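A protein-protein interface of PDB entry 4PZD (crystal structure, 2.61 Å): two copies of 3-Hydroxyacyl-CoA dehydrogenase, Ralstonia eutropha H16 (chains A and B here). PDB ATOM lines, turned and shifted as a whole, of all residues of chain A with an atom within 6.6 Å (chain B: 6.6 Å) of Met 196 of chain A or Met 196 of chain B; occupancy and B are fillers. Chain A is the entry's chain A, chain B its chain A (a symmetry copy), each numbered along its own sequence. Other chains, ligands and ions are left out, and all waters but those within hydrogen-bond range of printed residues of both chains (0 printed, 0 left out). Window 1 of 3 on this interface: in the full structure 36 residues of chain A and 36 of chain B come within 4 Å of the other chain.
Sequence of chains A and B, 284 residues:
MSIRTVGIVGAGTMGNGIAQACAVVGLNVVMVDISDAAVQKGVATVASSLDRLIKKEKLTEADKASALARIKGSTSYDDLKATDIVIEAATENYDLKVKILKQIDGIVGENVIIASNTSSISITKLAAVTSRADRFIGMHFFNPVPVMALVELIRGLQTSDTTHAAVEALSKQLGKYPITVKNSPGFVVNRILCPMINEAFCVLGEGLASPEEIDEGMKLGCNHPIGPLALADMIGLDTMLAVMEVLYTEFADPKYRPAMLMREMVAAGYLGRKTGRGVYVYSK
Met 196 of chain A touches just these residues of chain B: Ile 192 (3.5 Å) and Met 196 (3.5 Å). Of the printed residues of chain A, Met 196 of chain B touches Ile 192 and Met 196. Printed residues of chain A within 4 Å of Ile 192 of chain B: Met 196 (3.5 Å), Glu 199 (3.3 Å), Ala 200 (3.7 Å) and Met 218 (3.3 Å). Of the printed residues of chain A, Arg 191 of chain B touches Glu 199 (2.8 Å). Met 244 of chain B touches none of the printed residues of chain A. Phe 201 of chain A touches none of the printed residues of chain B. The nearest residue of chain B that does not touch Met 196 of chain A is Leu 193 of chain B (5.0 Å). The nearest printed residue of chain B that does not touch His 224 of chain A is Leu 193 of chain B (4.3 Å).
NE of Arg 191 of chain A is in salt-bridge range of OE2 of Glu 199 of chain B (2.8 Å). NE of Arg 191 of chain B is in salt-bridge range of OE2 of Glu 199 of chain A. SD of Met 196 of chain B sits close to SD of Met 196 of chain A, at 3.5 Å.
Ile 192 of chain A touches Met 196 of chain B, and with the chains exchanged Met 196 of chain A touches Ile 192 of chain B. Ile 192 of chain A touches Met 218 of chain B, and with the chains exchanged Met 218 of chain A touches Ile 192 of chain B. Met 196 of chain A touches its own counterpart, Met 196 of chain B. His 224 of chain A touches its own counterpart, His 224 of chain B. 19 positions are printed for both chains.
The backbone carbonyl oxygen (O) of Met 218 of chain A is in hydrogen-bond range of the backbone NH (N) of His 224 of chain A, at 3.4 Å. O of Met 218 of chain B sits at hydrogen-bond distance from N of His 224 of chain B (3.4 Å).
Ile 192 of chain A touches Met 196 of chain B. CG2 of Ile 192 of chain A touches CG of Glu 199 of chain B, 3.3 Å away. CG2 of Ile 192 of chain A touches N of Ala 200 of chain B, 3.7 Å away. Met 218 of chain B touches Ile 192 of chain A (SD to CG1, 3.3 Å). Met 196 of chain A touches Ile 192 of chain B. Glu 199 of chain A touches Ile 192 of chain B. N of Ala 200 of chain A touches CG2 of Ile 192 of chain B, 3.7 Å away. Met 218 of chain A touches Ile 192 of chain B. His 224 of chain B touches His 224 of chain A.
Printed residues of chain B that touch a printed residue of chain A: Arg 191, Ile 192, Met 196, Glu 199, Ala 200, Met 218 and His 224. Hydrophobic or aromatic side chains of chain B that line the printed part of chain A: Ile 192, Met 196, Met 218 and His 224. Hydrophobic or aromatic side chains of chain A within 4 Å of the printed part of chain B: Ile 192, Met 196, Met 218 and His 224. Among the printed residues, Asp or Glu carboxylates within 4 Å of a Lys or Arg side-chain nitrogen of the other chain: Arg 191 of chain A with Glu 199 of chain B (2.8 Å) and Glu 199 of chain A with Arg 191 of chain B (2.8 Å).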
ATOM      1  N   ASN A 190       9.089 -17.894  21.132  1.00  0.00           N
ATOM      2  CA  ASN A 190       8.448 -17.540  22.378  1.00  0.00           C
ATOM      3  C   ASN A 190       9.294 -16.573  23.185  1.00  0.00           C
ATOM      4  O   ASN A 190       8.763 -15.660  23.828  1.00  0.00           O
ATOM      5  CB  ASN A 190       8.042 -18.794  23.144  1.00  0.00           C
ATOM      6  CG  ASN A 190       6.822 -19.448  22.522  1.00  0.00           C
ATOM      7  OD1 ASN A 190       6.590 -20.640  22.655  1.00  0.00           O
ATOM      8  ND2 ASN A 190       6.038 -18.650  21.822  1.00  0.00           N
ATOM      9  N   ARG A 191      10.611 -16.723  23.069  1.00  0.00           N
ATOM     10  CA  ARG A 191      11.564 -15.829  23.743  1.00  0.00           C
ATOM     11  C   ARG A 191      11.371 -14.380  23.414  1.00  0.00           C
ATOM     12  O   ARG A 191      11.491 -13.539  24.293  1.00  0.00           O
ATOM     13  CB  ARG A 191      13.005 -16.221  23.429  1.00  0.00           C
ATOM     14  CG  ARG A 191      13.956 -15.926  24.578  1.00  0.00           C
ATOM     15  CD  ARG A 191      14.548 -14.594  24.339  1.00  0.00           C
ATOM     16  NE  ARG A 191      15.371 -14.068  25.405  1.00  0.00           N
ATOM     17  CZ  ARG A 191      16.653 -14.317  25.542  1.00  0.00           C
ATOM     18  NH1 ARG A 191      17.289 -15.227  24.791  1.00  0.00           N
ATOM     19  NH2 ARG A 191      17.297 -13.686  26.491  1.00  0.00           N
ATOM     20  N   ILE A 192      11.048 -14.041  22.182  1.00  0.00           N
ATOM     21  CA  ILE A 192      10.830 -12.625  21.943  1.00  0.00           C
ATOM     22  C   ILE A 192       9.366 -12.195  21.941  1.00  0.00           C
ATOM     23  O   ILE A 192       9.019 -11.122  22.452  1.00  0.00           O
ATOM     24  CB  ILE A 192      11.774 -12.034  20.845  1.00  0.00           C
ATOM     25  CG1 ILE A 192      11.730 -12.745  19.531  1.00  0.00           C
ATOM     26  CG2 ILE A 192      13.198 -12.194  21.327  1.00  0.00           C
ATOM     27  CD1 ILE A 192      13.105 -13.069  18.930  1.00  0.00           C
ATOM     28  N   LEU A 193       8.498 -13.055  21.438  1.00  0.00           N
ATOM     29  CA  LEU A 193       7.091 -12.745  21.422  1.00  0.00           C
ATOM     30  C   LEU A 193       6.569 -12.658  22.851  1.00  0.00           C
ATOM     31  O   LEU A 193       5.943 -11.673  23.217  1.00  0.00           O
ATOM     32  CB  LEU A 193       6.327 -13.800  20.627  1.00  0.00           C
ATOM     33  CG  LEU A 193       4.805 -13.569  20.566  1.00  0.00           C
ATOM     34  CD1 LEU A 193       4.487 -12.426  19.635  1.00  0.00           C
ATOM     35  CD2 LEU A 193       4.041 -14.815  20.137  1.00  0.00           C
ATOM     36  N   CYS A 194       6.835 -13.650  23.688  1.00  0.00           N
ATOM     37  CA  CYS A 194       6.036 -13.720  24.929  1.00  0.00           C
ATOM     38  C   CYS A 194       6.311 -12.592  25.908  1.00  0.00           C
ATOM     39  O   CYS A 194       5.391 -12.126  26.556  1.00  0.00           O
ATOM     40  CB  CYS A 194       6.102 -15.096  25.595  1.00  0.00           C
ATOM     41  SG  CYS A 194       5.339 -16.426  24.611  1.00  0.00           S
ATOM     42  N   PRO A 195       7.569 -12.125  25.998  1.00  0.00           N
ATOM     43  CA  PRO A 195       7.772 -10.937  26.876  1.00  0.00           C
ATOM     44  C   PRO A 195       7.119  -9.651  26.344  1.00  0.00           C
ATOM     45  O   PRO A 195       6.874  -8.711  27.088  1.00  0.00           O
ATOM     46  CB  PRO A 195       9.299 -10.828  26.994  1.00  0.00           C
ATOM     47  CG  PRO A 195       9.767 -12.244  26.809  1.00  0.00           C
ATOM     48  CD  PRO A 195       8.821 -12.875  25.803  1.00  0.00           C
ATOM     49  N   MET A 196       6.806  -9.629  25.065  1.00  0.00           N
ATOM     50  CA  MET A 196       6.056  -8.515  24.520  1.00  0.00           C
ATOM     51  C   MET A 196       4.603  -8.582  24.985  1.00  0.00           C
ATOM     52  O   MET A 196       4.056  -7.587  25.439  1.00  0.00           O
ATOM     53  CB  MET A 196       6.118  -8.563  23.016  1.00  0.00           C
ATOM     54  CG  MET A 196       5.761  -7.259  22.367  1.00  0.00           C
ATOM     55  SD  MET A 196       5.131  -7.637  20.747  1.00  0.00           S
ATOM     56  CE  MET A 196       3.462  -8.033  21.267  1.00  0.00           C
ATOM     57  N   ILE A 197       3.993  -9.765  24.889  1.00  0.00           N
ATOM     58  CA  ILE A 197       2.665  -9.946  25.421  1.00  0.00           C
ATOM     59  C   ILE A 197       2.696  -9.456  26.904  1.00  0.00           C
ATOM     60  O   ILE A 197       1.895  -8.593  27.332  1.00  0.00           O
ATOM     61  CB  ILE A 197       2.190 -11.419  25.369  1.00  0.00           C
ATOM     62  CG1 ILE A 197       2.402 -12.105  23.994  1.00  0.00           C
ATOM     63  CG2 ILE A 197       0.743 -11.504  25.802  1.00  0.00           C
ATOM     64  CD1 ILE A 197       1.885 -11.330  22.814  1.00  0.00           C
ATOM     65  N   ASN A 198       3.649  -9.983  27.660  1.00  0.00           N
ATOM     66  CA  ASN A 198       3.843  -9.579  29.053  1.00  0.00           C
ATOM     67  C   ASN A 198       3.925  -8.070  29.271  1.00  0.00           C
ATOM     68  O   ASN A 198       3.356  -7.537  30.221  1.00  0.00           O
ATOM     69  CB  ASN A 198       5.103 -10.225  29.624  1.00  0.00           C
ATOM     70  CG  ASN A 198       5.059 -10.335  31.129  1.00  0.00           C
ATOM     71  OD1 ASN A 198       5.955  -9.911  31.812  1.00  0.00           O
ATOM     72  ND2 ASN A 198       4.012 -10.935  31.639  1.00  0.00           N
ATOM     73  N   GLU A 199       4.620  -7.363  28.386  1.00  0.00           N
ATOM     74  CA  GLU A 199       4.674  -5.916  28.513  1.00  0.00           C
ATOM     75  C   GLU A 199       3.337  -5.251  28.298  1.00  0.00           C
ATOM     76  O   GLU A 199       3.104  -4.222  28.905  1.00  0.00           O
ATOM     77  CB  GLU A 199       5.680  -5.307  27.535  1.00  0.00           C
ATOM     78  CG  GLU A 199       6.267  -3.977  28.025  1.00  0.00           C
ATOM     79  CD  GLU A 199       7.039  -4.127  29.338  1.00  0.00           C
ATOM     80  OE1 GLU A 199       7.331  -5.284  29.718  1.00  0.00           O
ATOM     81  OE2 GLU A 199       7.368  -3.092  29.979  1.00  0.00           O
ATOM     82  N   ALA A 200       2.503  -5.780  27.388  1.00  0.00           N
ATOM     83  CA  ALA A 200       1.116  -5.298  27.208  1.00  0.00           C
ATOM     84  C   ALA A 200       0.368  -5.425  28.504  1.00  0.00           C
ATOM     85  O   ALA A 200      -0.311  -4.498  28.907  1.00  0.00           O
ATOM     86  CB  ALA A 200       0.371  -6.080  26.140  1.00  0.00           C
ATOM     87  N   PHE A 201       0.501  -6.559  29.180  1.00  0.00           N
ATOM     88  CA  PHE A 201      -0.182  -6.681  30.462  1.00  0.00           C
ATOM     89  C   PHE A 201       0.367  -5.668  31.441  1.00  0.00           C
ATOM     90  O   PHE A 201      -0.398  -5.111  32.218  1.00  0.00           O
ATOM     91  CB  PHE A 201      -0.116  -8.087  31.051  1.00  0.00           C
ATOM     92  CG  PHE A 201      -1.091  -9.018  30.447  1.00  0.00           C
ATOM     93  CD1 PHE A 201      -0.840  -9.604  29.230  1.00  0.00           C
ATOM     94  CD2 PHE A 201      -2.296  -9.292  31.080  1.00  0.00           C
ATOM     95  CE1 PHE A 201      -1.753 -10.475  28.664  1.00  0.00           C
ATOM     96  CE2 PHE A 201      -3.224 -10.160  30.520  1.00  0.00           C
ATOM     97  CZ  PHE A 201      -2.945 -10.763  29.314  1.00  0.00           C
ATOM     98  N   MET A 218      -1.045  -1.486  18.560  1.00  0.00           N
ATOM     99  CA  MET A 218      -0.090  -2.435  18.001  1.00  0.00           C
ATOM    100  C   MET A 218      -0.450  -2.962  16.598  1.00  0.00           C
ATOM    101  O   MET A 218       0.485  -3.260  15.809  1.00  0.00           O
ATOM    102  CB  MET A 218       0.129  -3.608  18.963  1.00  0.00           C
ATOM    103  CG  MET A 218       0.678  -3.237  20.342  1.00  0.00           C
ATOM    104  SD  MET A 218       2.221  -2.285  20.425  1.00  0.00           S
ATOM    105  CE  MET A 218       3.278  -3.240  19.346  1.00  0.00           C
ATOM    106  N   HIS A 224       0.612  -5.423  13.133  1.00  0.00           N
ATOM    107  CA  HIS A 224       0.567  -6.785  13.668  1.00  0.00           C
ATOM    108  C   HIS A 224      -0.839  -7.268  13.358  1.00  0.00           C
ATOM    109  O   HIS A 224      -1.772  -6.520  13.525  1.00  0.00           O
ATOM    110  CB  HIS A 224       0.783  -6.833  15.197  1.00  0.00           C
ATOM    111  CG  HIS A 224       2.192  -6.582  15.636  1.00  0.00           C
ATOM    112  ND1 HIS A 224       2.545  -6.483  16.968  1.00  0.00           N
ATOM    113  CD2 HIS A 224       3.330  -6.385  14.930  1.00  0.00           C
ATOM    114  CE1 HIS A 224       3.845  -6.257  17.066  1.00  0.00           C
ATOM    115  NE2 HIS A 224       4.342  -6.191  15.843  1.00  0.00           N
ATOM    116  N   GLY A 227      -3.683  -8.079  18.107  1.00  0.00           N
ATOM    117  CA  GLY A 227      -3.130  -7.323  19.212  1.00  0.00           C
ATOM    118  C   GLY A 227      -2.673  -8.256  20.324  1.00  0.00           C
ATOM    119  O   GLY A 227      -3.314  -9.292  20.571  1.00  0.00           O
ATOM    120  N   PRO A 228      -1.599  -7.867  21.051  1.00  0.00           N
ATOM    121  CA  PRO A 228      -1.025  -8.771  22.027  1.00  0.00           C
ATOM    122  C   PRO A 228      -2.050  -9.261  23.055  1.00  0.00           C
ATOM    123  O   PRO A 228      -2.026 -10.436  23.408  1.00  0.00           O
ATOM    124  CB  PRO A 228       0.091  -7.958  22.668  1.00  0.00           C
ATOM    125  CG  PRO A 228      -0.298  -6.544  22.479  1.00  0.00           C
ATOM    126  CD  PRO A 228      -1.185  -6.474  21.273  1.00  0.00           C
ATOM    127  N   LEU A 231      -4.274 -11.826  21.496  1.00  0.00           N
ATOM    128  CA  LEU A 231      -3.407 -12.979  21.243  1.00  0.00           C
ATOM    129  C   LEU A 231      -3.186 -13.777  22.513  1.00  0.00           C
ATOM    130  O   LEU A 231      -3.078 -15.010  22.469  1.00  0.00           O
ATOM    131  CB  LEU A 231      -2.072 -12.507  20.685  1.00  0.00           C
ATOM    132  CG  LEU A 231      -1.055 -13.593  20.329  1.00  0.00           C
ATOM    133  CD1 LEU A 231      -1.685 -14.689  19.470  1.00  0.00           C
ATOM    134  CD2 LEU A 231       0.164 -12.973  19.648  1.00  0.00           C
ATOM    135  N   MET A 240       0.651 -18.527  28.723  1.00  0.00           N
ATOM    136  CA  MET A 240       1.475 -17.319  28.847  1.00  0.00           C
ATOM    137  C   MET A 240       2.264 -17.180  30.173  1.00  0.00           C
ATOM    138  O   MET A 240       3.496 -17.013  30.175  1.00  0.00           O
ATOM    139  CB  MET A 240       0.610 -16.060  28.702  1.00  0.00           C
ATOM    140  CG  MET A 240       0.350 -15.592  27.280  1.00  0.00           C
ATOM    141  SD  MET A 240       1.729 -15.553  26.091  1.00  0.00           S
ATOM    142  CE  MET A 240       2.936 -14.551  26.964  1.00  0.00           C
ATOM    143  N   MET A 244       6.402 -17.238  30.816  1.00  0.00           N
ATOM    144  CA  MET A 244       7.129 -16.231  31.586  1.00  0.00           C
ATOM    145  C   MET A 244       7.749 -16.810  32.836  1.00  0.00           C
ATOM    146  O   MET A 244       8.823 -16.469  33.188  1.00  0.00           O
ATOM    147  CB  MET A 244       6.222 -15.041  31.939  1.00  0.00           C
ATOM    148  CG  MET A 244       5.726 -14.212  30.743  1.00  0.00           C
ATOM    149  SD  MET A 244       7.025 -13.448  29.732  1.00  0.00           S
ATOM    150  CE  MET A 244       7.195 -14.807  28.630  1.00  0.00           C
ATOM    151  N   ASN B 190       5.784   2.397  21.426  1.00  0.00           N
ATOM    152  CA  ASN B 190       7.202   2.150  21.560  1.00  0.00           C
ATOM    153  C   ASN B 190       7.511   1.342  22.805  1.00  0.00           C
ATOM    154  O   ASN B 190       8.396   0.476  22.788  1.00  0.00           O
ATOM    155  CB  ASN B 190       7.983   3.455  21.460  1.00  0.00           C
ATOM    156  CG  ASN B 190       8.046   3.951  20.026  1.00  0.00           C
ATOM    157  OD1 ASN B 190       8.202   5.133  19.758  1.00  0.00           O
ATOM    158  ND2 ASN B 190       7.911   3.026  19.094  1.00  0.00           N
ATOM    159  N   ARG B 191       6.718   1.564  23.849  1.00  0.00           N
ATOM    160  CA  ARG B 191       6.854   0.818  25.109  1.00  0.00           C
ATOM    161  C   ARG B 191       6.769  -0.668  24.946  1.00  0.00           C
ATOM    162  O   ARG B 191       7.511  -1.391  25.596  1.00  0.00           O
ATOM    163  CB  ARG B 191       5.811   1.266  26.130  1.00  0.00           C
ATOM    164  CG  ARG B 191       6.313   1.170  27.562  1.00  0.00           C
ATOM    165  CD  ARG B 191       5.888  -0.139  28.099  1.00  0.00           C
ATOM    166  NE  ARG B 191       6.401  -0.482  29.406  1.00  0.00           N
ATOM    167  CZ  ARG B 191       5.834  -0.135  30.538  1.00  0.00           C
ATOM    168  NH1 ARG B 191       4.805   0.720  30.590  1.00  0.00           N
ATOM    169  NH2 ARG B 191       6.348  -0.607  31.646  1.00  0.00           N
ATOM    170  N   ILE B 192       5.911  -1.170  24.081  1.00  0.00           N
ATOM    171  CA  ILE B 192       5.914  -2.614  23.937  1.00  0.00           C
ATOM    172  C   ILE B 192       6.703  -3.138  22.741  1.00  0.00           C
ATOM    173  O   ILE B 192       7.389  -4.164  22.832  1.00  0.00           O
ATOM    174  CB  ILE B 192       4.527  -3.267  24.249  1.00  0.00           C
ATOM    175  CG1 ILE B 192       3.385  -2.718  23.456  1.00  0.00           C
ATOM    176  CG2 ILE B 192       4.186  -2.959  25.689  1.00  0.00           C
ATOM    177  CD1 ILE B 192       2.136  -2.378  24.281  1.00  0.00           C
ATOM    178  N   LEU B 193       6.671  -2.401  21.644  1.00  0.00           N
ATOM    179  CA  LEU B 193       7.409  -2.802  20.475  1.00  0.00           C
ATOM    180  C   LEU B 193       8.904  -2.756  20.772  1.00  0.00           C
ATOM    181  O   LEU B 193       9.606  -3.730  20.542  1.00  0.00           O
ATOM    182  CB  LEU B 193       7.062  -1.900  19.294  1.00  0.00           C
ATOM    183  CG  LEU B 193       7.817  -2.237  17.994  1.00  0.00           C
ATOM    184  CD1 LEU B 193       7.266  -3.499  17.381  1.00  0.00           C
ATOM    185  CD2 LEU B 193       7.769  -1.102  16.979  1.00  0.00           C
ATOM    186  N   CYS B 194       9.413  -1.658  21.311  1.00  0.00           N
ATOM    187  CA  CYS B 194      10.880  -1.497  21.257  1.00  0.00           C
ATOM    188  C   CYS B 194      11.645  -2.482  22.125  1.00  0.00           C
ATOM    189  O   CYS B 194      12.705  -2.928  21.727  1.00  0.00           O
ATOM    190  CB  CYS B 194      11.322  -0.050  21.494  1.00  0.00           C
ATOM    191  SG  CYS B 194      10.795   1.102  20.186  1.00  0.00           S
ATOM    192  N   PRO B 195      11.097  -2.852  23.296  1.00  0.00           N
ATOM    193  CA  PRO B 195      11.816  -3.913  24.056  1.00  0.00           C
ATOM    194  C   PRO B 195      11.788  -5.292  23.378  1.00  0.00           C
ATOM    195  O   PRO B 195      12.611  -6.153  23.661  1.00  0.00           O
ATOM    196  CB  PRO B 195      11.129  -3.906  25.429  1.00  0.00           C
ATOM    197  CG  PRO B 195      10.635  -2.494  25.567  1.00  0.00           C
ATOM    198  CD  PRO B 195      10.229  -2.049  24.174  1.00  0.00           C
ATOM    199  N   MET B 196      10.864  -5.484  22.460  1.00  0.00           N
ATOM    200  CA  MET B 196      10.864  -6.701  21.673  1.00  0.00           C
ATOM    201  C   MET B 196      12.012  -6.675  20.666  1.00  0.00           C
ATOM    202  O   MET B 196      12.749  -7.644  20.549  1.00  0.00           O
ATOM    203  CB  MET B 196       9.548  -6.825  20.950  1.00  0.00           C
ATOM    204  CG  MET B 196       9.268  -8.217  20.467  1.00  0.00           C
ATOM    205  SD  MET B 196       8.192  -8.072  19.058  1.00  0.00           S
ATOM    206  CE  MET B 196       9.478  -7.729  17.856  1.00  0.00           C
ATOM    207  N   ILE B 197      12.170  -5.555  19.959  1.00  0.00           N
ATOM    208  CA  ILE B 197      13.302  -5.401  19.080  1.00  0.00           C
ATOM    209  C   ILE B 197      14.580  -5.711  19.923  1.00  0.00           C
ATOM    210  O   ILE B 197      15.418  -6.569  19.561  1.00  0.00           O
ATOM    211  CB  ILE B 197      13.409  -3.978  18.477  1.00  0.00           C
ATOM    212  CG1 ILE B 197      12.083  -3.445  17.875  1.00  0.00           C
ATOM    213  CG2 ILE B 197      14.525  -3.939  17.458  1.00  0.00           C
ATOM    214  CD1 ILE B 197      11.399  -4.384  16.921  1.00  0.00           C
ATOM    215  N   ASN B 198      14.694  -5.038  21.059  1.00  0.00           N
ATOM    216  CA  ASN B 198      15.804  -5.262  21.985  1.00  0.00           C
ATOM    217  C   ASN B 198      16.047  -6.727  22.342  1.00  0.00           C
ATOM    218  O   ASN B 198      17.186  -7.182  22.406  1.00  0.00           O
ATOM    219  CB  ASN B 198      15.593  -4.473  23.274  1.00  0.00           C
ATOM    220  CG  ASN B 198      16.889  -4.191  23.993  1.00  0.00           C
ATOM    221  OD1 ASN B 198      17.032  -4.473  25.155  1.00  0.00           O
ATOM    222  ND2 ASN B 198      17.829  -3.606  23.293  1.00  0.00           N
ATOM    223  N   GLU B 199      14.978  -7.486  22.563  1.00  0.00           N
ATOM    224  CA  GLU B 199      15.153  -8.901  22.843  1.00  0.00           C
ATOM    225  C   GLU B 199      15.710  -9.673  21.672  1.00  0.00           C
ATOM    226  O   GLU B 199      16.416 -10.637  21.905  1.00  0.00           O
ATOM    227  CB  GLU B 199      13.836  -9.553  23.270  1.00  0.00           C
ATOM    228  CG  GLU B 199      14.036 -10.775  24.176  1.00  0.00           C
ATOM    229  CD  GLU B 199      14.741 -10.422  25.487  1.00  0.00           C
ATOM    230  OE1 GLU B 199      14.837  -9.212  25.795  1.00  0.00           O
ATOM    231  OE2 GLU B 199      15.184 -11.351  26.216  1.00  0.00           O
ATOM    232  N   ALA B 200      15.335  -9.310  20.435  1.00  0.00           N
ATOM    233  CA  ALA B 200      15.935  -9.900  19.219  1.00  0.00           C
ATOM    234  C   ALA B 200      17.419  -9.671  19.230  1.00  0.00           C
ATOM    235  O   ALA B 200      18.177 -10.588  18.966  1.00  0.00           O
ATOM    236  CB  ALA B 200      15.363  -9.299  17.946  1.00  0.00           C
ATOM    237  N   PHE B 201      17.851  -8.460  19.557  1.00  0.00           N
ATOM    238  CA  PHE B 201      19.291  -8.234  19.617  1.00  0.00           C
ATOM    239  C   PHE B 201      19.905  -9.088  20.704  1.00  0.00           C
ATOM    240  O   PHE B 201      21.001  -9.599  20.515  1.00  0.00           O
ATOM    241  CB  PHE B 201      19.665  -6.768  19.811  1.00  0.00           C
ATOM    242  CG  PHE B 201      19.597  -5.980  18.563  1.00  0.00           C
ATOM    243  CD1 PHE B 201      18.392  -5.525  18.085  1.00  0.00           C
ATOM    244  CD2 PHE B 201      20.745  -5.714  17.829  1.00  0.00           C
ATOM    245  CE1 PHE B 201      18.328  -4.788  16.917  1.00  0.00           C
ATOM    246  CE2 PHE B 201      20.695  -4.981  16.652  1.00  0.00           C
ATOM    247  CZ  PHE B 201      19.483  -4.505  16.202  1.00  0.00           C
ATOM    248  N   MET B 218       9.951 -14.829  13.399  1.00  0.00           N
ATOM    249  CA  MET B 218       8.914 -13.891  13.815  1.00  0.00           C
ATOM    250  C   MET B 218       7.873 -13.556  12.730  1.00  0.00           C
ATOM    251  O   MET B 218       6.695 -13.292  13.087  1.00  0.00           O
ATOM    252  CB  MET B 218       9.542 -12.602  14.357  1.00  0.00           C
ATOM    253  CG  MET B 218      10.455 -12.772  15.573  1.00  0.00           C
ATOM    254  SD  MET B 218       9.784 -13.605  17.040  1.00  0.00           S
ATOM    255  CE  MET B 218       8.253 -12.715  17.277  1.00  0.00           C
ATOM    256  N   HIS B 224       4.209 -11.452  11.573  1.00  0.00           N
ATOM    257  CA  HIS B 224       4.598 -10.043  11.650  1.00  0.00           C
ATOM    258  C   HIS B 224       5.035  -9.693  10.238  1.00  0.00           C
ATOM    259  O   HIS B 224       5.712 -10.476   9.617  1.00  0.00           O
ATOM    260  CB  HIS B 224       5.784  -9.802  12.610  1.00  0.00           C
ATOM    261  CG  HIS B 224       5.441  -9.908  14.063  1.00  0.00           C
ATOM    262  ND1 HIS B 224       6.398  -9.826  15.057  1.00  0.00           N
ATOM    263  CD2 HIS B 224       4.261 -10.110  14.694  1.00  0.00           C
ATOM    264  CE1 HIS B 224       5.818  -9.955  16.240  1.00  0.00           C
ATOM    265  NE2 HIS B 224       4.523 -10.130  16.045  1.00  0.00           N
ATOM    266  N   GLY B 227      10.505  -8.522  10.152  1.00  0.00           N
ATOM    267  CA  GLY B 227      11.207  -9.105  11.277  1.00  0.00           C
ATOM    268  C   GLY B 227      11.855  -8.021  12.126  1.00  0.00           C
ATOM    269  O   GLY B 227      12.330  -7.008  11.586  1.00  0.00           O
ATOM    270  N   PRO B 228      11.939  -8.251  13.458  1.00  0.00           N
ATOM    271  CA  PRO B 228      12.412  -7.203  14.339  1.00  0.00           C
ATOM    272  C   PRO B 228      13.789  -6.666  13.936  1.00  0.00           C
ATOM    273  O   PRO B 228      13.999  -5.458  13.999  1.00  0.00           O
ATOM    274  CB  PRO B 228      12.430  -7.861  15.713  1.00  0.00           C
ATOM    275  CG  PRO B 228      12.565  -9.310  15.450  1.00  0.00           C
ATOM    276  CD  PRO B 228      12.004  -9.578  14.086  1.00  0.00           C
ATOM    277  N   LEU B 231      13.451  -4.451  10.947  1.00  0.00           N
ATOM    278  CA  LEU B 231      12.708  -3.282  11.420  1.00  0.00           C
ATOM    279  C   LEU B 231      13.621  -2.328  12.165  1.00  0.00           C
ATOM    280  O   LEU B 231      13.447  -1.105  12.090  1.00  0.00           O
ATOM    281  CB  LEU B 231      11.569  -3.727  12.325  1.00  0.00           C
ATOM    282  CG  LEU B 231      10.666  -2.625  12.882  1.00  0.00           C
ATOM    283  CD1 LEU B 231      10.190  -1.681  11.779  1.00  0.00           C
ATOM    284  CD2 LEU B 231       9.492  -3.239  13.644  1.00  0.00           C
ATOM    285  N   MET B 240      16.598   3.357  18.054  1.00  0.00           N
ATOM    286  CA  MET B 240      16.353   2.228  18.960  1.00  0.00           C
ATOM    287  C   MET B 240      17.081   2.297  20.326  1.00  0.00           C
ATOM    288  O   MET B 240      16.452   2.212  21.395  1.00  0.00           O
ATOM    289  CB  MET B 240      16.763   0.906  18.297  1.00  0.00           C
ATOM    290  CG  MET B 240      15.719   0.260  17.402  1.00  0.00           C
ATOM    291  SD  MET B 240      13.991   0.173  17.972  1.00  0.00           S
ATOM    292  CE  MET B 240      14.173  -0.639  19.563  1.00  0.00           C
ATOM    293  N   MET B 244      15.469   2.701  24.171  1.00  0.00           N
ATOM    294  CA  MET B 244      15.813   1.841  25.301  1.00  0.00           C
ATOM    295  C   MET B 244      16.516   2.601  26.401  1.00  0.00           C
ATOM    296  O   MET B 244      16.278   2.376  27.535  1.00  0.00           O
ATOM    297  CB  MET B 244      16.663   0.643  24.849  1.00  0.00           C
ATOM    298  CG  MET B 244      15.958  -0.351  23.911  1.00  0.00           C
ATOM    299  SD  MET B 244      14.471  -1.140  24.589  1.00  0.00           S
ATOM    300  CE  MET B 244      13.356   0.089  24.011  1.00  0.00           C
